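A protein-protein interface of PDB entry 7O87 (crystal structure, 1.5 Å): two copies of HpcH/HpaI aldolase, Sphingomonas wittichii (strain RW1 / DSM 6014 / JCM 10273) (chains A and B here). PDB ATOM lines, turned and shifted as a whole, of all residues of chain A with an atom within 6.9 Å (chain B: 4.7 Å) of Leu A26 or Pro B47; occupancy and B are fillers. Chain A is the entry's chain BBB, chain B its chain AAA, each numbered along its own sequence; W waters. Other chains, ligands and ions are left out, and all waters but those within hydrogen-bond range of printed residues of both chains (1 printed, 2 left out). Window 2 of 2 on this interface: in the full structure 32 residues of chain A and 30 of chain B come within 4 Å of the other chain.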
ATOM      1  N   PRO A  23      -4.761 -30.996 -14.163  1.00  0.00           N
ATOM      2  CA  PRO A  23      -4.546 -32.040 -13.167  1.00  0.00           C
ATOM      3  C   PRO A  23      -3.562 -31.647 -12.058  1.00  0.00           C
ATOM      4  O   PRO A  23      -2.739 -30.772 -12.272  1.00  0.00           O
ATOM      5  CB  PRO A  23      -3.951 -33.181 -13.976  1.00  0.00           C
ATOM      6  CG  PRO A  23      -3.278 -32.500 -15.146  1.00  0.00           C
ATOM      7  CD  PRO A  23      -4.129 -31.291 -15.459  1.00  0.00           C
ATOM      8  N   GLY A  24      -3.726 -32.243 -10.878  1.00  0.00           N
ATOM      9  CA  GLY A  24      -2.763 -32.129  -9.762  1.00  0.00           C
ATOM     10  C   GLY A  24      -3.446 -31.704  -8.475  1.00  0.00           C
ATOM     11  O   GLY A  24      -4.565 -31.198  -8.542  1.00  0.00           O
ATOM     12  N   THR A  25      -2.771 -31.868  -7.334  1.00  0.00           N
ATOM     13  CA  THR A  25      -3.373 -31.713  -5.983  1.00  0.00           C
ATOM     14  C   THR A  25      -3.042 -30.352  -5.383  1.00  0.00           C
ATOM     15  O   THR A  25      -3.832 -29.880  -4.504  1.00  0.00           O
ATOM     16  CB  THR A  25      -2.866 -32.809  -5.059  1.00  0.00           C
ATOM     17  OG1 THR A  25      -1.440 -32.861  -5.139  1.00  0.00           O
ATOM     18  CG2 THR A  25      -3.466 -34.156  -5.414  1.00  0.00           C
ATOM     19  N   LEU A  26      -1.948 -29.717  -5.802  1.00  0.00           N
ATOM     20  CA  LEU A  26      -1.461 -28.506  -5.086  1.00  0.00           C
ATOM     21  C   LEU A  26      -2.412 -27.340  -5.368  1.00  0.00           C
ATOM     22  O   LEU A  26      -2.882 -26.718  -4.370  1.00  0.00           O
ATOM     23  CB  LEU A  26       0.001 -28.215  -5.435  1.00  0.00           C
ATOM     24  CG  LEU A  26       0.645 -27.036  -4.717  1.00  0.00           C
ATOM     25  CD1 LEU A  26       0.401 -27.117  -3.225  1.00  0.00           C
ATOM     26  CD2 LEU A  26       2.122 -26.912  -5.043  1.00  0.00           C
ATOM     27  N   HIS A  27      -2.717 -27.018  -6.624  1.00  0.00           N
ATOM     28  CA  HIS A  27      -3.691 -25.926  -6.900  1.00  0.00           C
ATOM     29  C   HIS A  27      -5.095 -26.338  -6.417  1.00  0.00           C
ATOM     30  O   HIS A  27      -5.889 -25.445  -6.040  1.00  0.00           O
ATOM     31  CB  HIS A  27      -3.649 -25.499  -8.369  1.00  0.00           C
ATOM     32  CG  HIS A  27      -4.268 -26.478  -9.289  1.00  0.00           C
ATOM     33  ND1 HIS A  27      -3.792 -27.748  -9.356  1.00  0.00           N
ATOM     34  CD2 HIS A  27      -5.282 -26.382 -10.184  1.00  0.00           C
ATOM     35  CE1 HIS A  27      -4.478 -28.422 -10.247  1.00  0.00           C
ATOM     36  NE2 HIS A  27      -5.427 -27.614 -10.745  1.00  0.00           N
ATOM     37  N   ALA A  28      -5.441 -27.633  -6.421  1.00  0.00           N
ATOM     38  CA  ALA A  28      -6.791 -28.124  -6.003  1.00  0.00           C
ATOM     39  C   ALA A  28      -7.009 -27.792  -4.526  1.00  0.00           C
ATOM     40  O   ALA A  28      -8.065 -27.158  -4.183  1.00  0.00           O
ATOM     41  CB  ALA A  28      -6.948 -29.594  -6.276  1.00  0.00           C
ATOM     42  N   GLU A  29      -6.037 -28.134  -3.676  1.00  0.00           N
ATOM     43  CA  GLU A  29      -6.090 -27.786  -2.230  1.00  0.00           C
ATOM     44  C   GLU A  29      -6.057 -26.269  -2.086  1.00  0.00           C
ATOM     45  O   GLU A  29      -6.861 -25.731  -1.301  1.00  0.00           O
ATOM     46  CB  GLU A  29      -4.966 -28.475  -1.449  1.00  0.00           C
ATOM     47  CG  GLU A  29      -5.048 -28.248   0.054  1.00  0.00           C
ATOM     48  CD  GLU A  29      -3.845 -28.649   0.890  1.00  0.00           C
ATOM     49  OE1 GLU A  29      -3.078 -29.484   0.425  1.00  0.00           O
ATOM     50  OE2 GLU A  29      -3.709 -28.142   2.021  1.00  0.00           O
ATOM     51  N   ALA A  30      -5.130 -25.583  -2.757  1.00  0.00           N
ATOM     52  CA  ALA A  30      -4.977 -24.117  -2.600  1.00  0.00           C
ATOM     53  C   ALA A  30      -6.303 -23.396  -2.944  1.00  0.00           C
ATOM     54  O   ALA A  30      -6.661 -22.420  -2.235  1.00  0.00           O
ATOM     55  CB  ALA A  30      -3.840 -23.630  -3.463  1.00  0.00           C
ATOM     56  N   LEU A  31      -7.017 -23.782  -4.018  1.00  0.00           N
ATOM     57  CA  LEU A  31      -8.300 -23.108  -4.402  1.00  0.00           C
ATOM     58  C   LEU A  31      -9.409 -23.524  -3.427  1.00  0.00           C
ATOM     59  O   LEU A  31     -10.199 -22.679  -2.999  1.00  0.00           O
ATOM     60  CB  LEU A  31      -8.634 -23.440  -5.864  1.00  0.00           C
ATOM     61  CG  LEU A  31      -7.635 -22.873  -6.874  1.00  0.00           C
ATOM     62  CD1 LEU A  31      -7.991 -23.259  -8.300  1.00  0.00           C
ATOM     63  CD2 LEU A  31      -7.506 -21.375  -6.739  1.00  0.00           C
ATOM     64  N   ALA A  59      -7.544 -33.855  -2.039  1.00  0.00           N
ATOM     65  CA  ALA A  59      -6.945 -32.514  -1.829  1.00  0.00           C
ATOM     66  C   ALA A  59      -8.037 -31.459  -1.601  1.00  0.00           C
ATOM     67  O   ALA A  59      -7.919 -30.585  -0.706  1.00  0.00           O
ATOM     68  CB  ALA A  59      -6.082 -32.161  -3.010  1.00  0.00           C
ATOM     69  N   GLN B  21       5.439 -24.262 -10.575  1.00  0.00           N
ATOM     70  CA  GLN B  21       5.500 -25.094  -9.354  1.00  0.00           C
ATOM     71  C   GLN B  21       4.423 -26.161  -9.419  1.00  0.00           C
ATOM     72  O   GLN B  21       4.391 -27.017  -8.532  1.00  0.00           O
ATOM     73  CB  GLN B  21       5.342 -24.207  -8.118  1.00  0.00           C
ATOM     74  CG  GLN B  21       6.628 -23.478  -7.796  1.00  0.00           C
ATOM     75  CD  GLN B  21       6.387 -22.280  -6.916  1.00  0.00           C
ATOM     76  OE1 GLN B  21       5.246 -21.921  -6.622  1.00  0.00           O
ATOM     77  NE2 GLN B  21       7.481 -21.686  -6.469  1.00  0.00           N
ATOM     78  N   LEU B  22       3.556 -26.091 -10.433  1.00  0.00           N
ATOM     79  CA  LEU B  22       2.453 -27.051 -10.623  1.00  0.00           C
ATOM     80  C   LEU B  22       2.873 -28.080 -11.669  1.00  0.00           C
ATOM     81  O   LEU B  22       3.267 -27.731 -12.773  1.00  0.00           O
ATOM     82  CB  LEU B  22       1.199 -26.275 -11.040  1.00  0.00           C
ATOM     83  CG  LEU B  22       0.729 -25.270  -9.996  1.00  0.00           C
ATOM     84  CD1 LEU B  22      -0.453 -24.476 -10.524  1.00  0.00           C
ATOM     85  CD2 LEU B  22       0.400 -25.950  -8.668  1.00  0.00           C
ATOM     86  N   PRO B  23       2.748 -29.390 -11.398  1.00  0.00           N
ATOM     87  CA  PRO B  23       3.012 -30.405 -12.418  1.00  0.00           C
ATOM     88  C   PRO B  23       1.959 -30.363 -13.544  1.00  0.00           C
ATOM     89  O   PRO B  23       0.823 -29.942 -13.300  1.00  0.00           O
ATOM     90  CB  PRO B  23       2.926 -31.736 -11.678  1.00  0.00           C
ATOM     91  CG  PRO B  23       2.166 -31.416 -10.420  1.00  0.00           C
ATOM     92  CD  PRO B  23       2.317 -29.941 -10.115  1.00  0.00           C
ATOM     93  N   SER B  46       8.404 -27.478  -5.055  1.00  0.00           N
ATOM     94  CA  SER B  46       7.217 -28.009  -5.756  1.00  0.00           C
ATOM     95  C   SER B  46       7.133 -29.496  -5.479  1.00  0.00           C
ATOM     96  O   SER B  46       8.099 -30.088  -5.019  1.00  0.00           O
ATOM     97  CB  SER B  46       7.315 -27.831  -7.255  1.00  0.00           C
ATOM     98  OG  SER B  46       8.195 -28.835  -7.753  1.00  0.00           O
ATOM     99  N   PRO B  47       6.001 -30.135  -5.814  1.00  0.00           N
ATOM    100  CA  PRO B  47       5.898 -31.602  -5.765  1.00  0.00           C
ATOM    101  C   PRO B  47       6.273 -32.349  -7.061  1.00  0.00           C
ATOM    102  O   PRO B  47       6.059 -33.574  -7.150  1.00  0.00           O
ATOM    103  CB  PRO B  47       4.415 -31.793  -5.434  1.00  0.00           C
ATOM    104  CG  PRO B  47       3.722 -30.628  -6.115  1.00  0.00           C
ATOM    105  CD  PRO B  47       4.718 -29.479  -6.072  1.00  0.00           C
ATOM    106  N   ILE B  48       6.941 -31.655  -7.972  1.00  0.00           N
ATOM    107  CA  ILE B  48       7.288 -32.181  -9.325  1.00  0.00           C
ATOM    108  C   ILE B  48       8.464 -33.164  -9.173  1.00  0.00           C
ATOM    109  O   ILE B  48       9.554 -32.697  -8.784  1.00  0.00           O
ATOM    110  CB  ILE B  48       7.603 -31.012 -10.279  1.00  0.00           C
ATOM    111  CG1 ILE B  48       6.439 -30.018 -10.329  1.00  0.00           C
ATOM    112  CG2 ILE B  48       7.961 -31.533 -11.660  1.00  0.00           C
ATOM    113  CD1 ILE B  48       6.678 -28.757 -11.147  1.00  0.00           C
ATOM    114  N   ASP B  49       8.277 -34.438  -9.538  1.00  0.00           N
ATOM    115  CA  ASP B  49       9.375 -35.437  -9.555  1.00  0.00           C
ATOM    116  C   ASP B  49       9.884 -35.613 -10.981  1.00  0.00           C
ATOM    117  O   ASP B  49       9.328 -35.005 -11.878  1.00  0.00           O
ATOM    118  CB  ASP B  49       8.950 -36.762  -8.923  1.00  0.00           C
ATOM    119  CG  ASP B  49       8.132 -37.698  -9.797  1.00  0.00           C
ATOM    120  OD1 ASP B  49       7.606 -37.258 -10.850  1.00  0.00           O
ATOM    121  OD2 ASP B  49       7.996 -38.886  -9.402  1.00  0.00           O
ATOM    122  N   GLN B  52       7.409 -36.400 -13.698  1.00  0.00           N
ATOM    123  CA  GLN B  52       6.474 -35.292 -14.059  1.00  0.00           C
ATOM    124  C   GLN B  52       7.215 -34.191 -14.833  1.00  0.00           C
ATOM    125  O   GLN B  52       6.601 -33.598 -15.740  1.00  0.00           O
ATOM    126  CB  GLN B  52       5.772 -34.762 -12.819  1.00  0.00           C
ATOM    127  CG  GLN B  52       4.808 -35.761 -12.219  1.00  0.00           C
ATOM    128  CD  GLN B  52       4.188 -35.222 -10.954  1.00  0.00           C
ATOM    129  OE1 GLN B  52       4.865 -34.955  -9.959  1.00  0.00           O
ATOM    130  NE2 GLN B  52       2.871 -35.055 -10.999  1.00  0.00           N
ATOM    131  N   LEU B 235       1.402 -20.966  -9.418  1.00  0.00           N
ATOM    132  CA  LEU B 235       0.457 -21.180  -8.284  1.00  0.00           C
ATOM    133  C   LEU B 235       0.099 -19.827  -7.645  1.00  0.00           C
ATOM    134  O   LEU B 235      -1.080 -19.611  -7.358  1.00  0.00           O
ATOM    135  CB  LEU B 235       1.067 -22.138  -7.255  1.00  0.00           C
ATOM    136  CG  LEU B 235       0.309 -22.290  -5.937  1.00  0.00           C
ATOM    137  CD1 LEU B 235      -1.067 -22.915  -6.149  1.00  0.00           C
ATOM    138  CD2 LEU B 235       1.115 -23.115  -4.944  1.00  0.00           C
HETATM  139  O   HOH W   1      -0.317 -32.850 -12.881  1.00  0.00           O
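Pro A23 touches its own counterpart, Pro B23.
1 position is printed for both chains.
Of the 6 pairs that touch across the chains among the printed residues, 1 has its exchanged pair printed and touching as well.
OE1 of Gln B52 sits close to O of Pro B47, at 3.4 Å.
Among the printed residues, merely in contact across the chains: Leu A26 with Pro B47, Pro A23 with Pro B23, His A27 with Leu B22, Ala A30 with Leu B235, Leu A26 with Leu B235 and Leu A26 with Leu B22.
Of chain B, only Leu B22, Pro B47 and Leu B235 come within 4 Å of Leu A26.
Printed residues of chain B within 4 Å of His A27: Leu B22.
Ala A28 touches none of the printed residues of chain B.
Of the printed residues of chain B, Ala A30 touches Leu B235 (3.9 Å).
Of the printed residues of chain A, Pro B23 touches Pro A23.
Pro B47 touches just one residue of chain A: Leu A26.
Of the printed residues of chain A, Leu B235 touches Leu A26 (3.9 Å) and Ala A30 (3.9 Å).
Water W1 bridges O of Pro B23 and O of Pro A23.
Of the 10 printed residues of chain A, 4 touch a printed residue of chain B.
Printed residues of chain A that touch a printed residue of chain B: Pro A23, Leu A26, His A27 and Ala A30.
Hydrophobic or aromatic side chains of chain A that line the printed part of chain B: Leu A26, His A27 and Ala A30.
Along chain A the printed residues that touch a printed residue of chain B span positions 23 to 30.
Of the 9 printed residues of chain B, 4 touch a printed residue of chain A.
Hydrophobic or aromatic side chains of chain B that line the printed part of chain A: Leu B22, Pro B47 and Leu B235.
Among the printed residues, 6 pairs touch across the chains.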
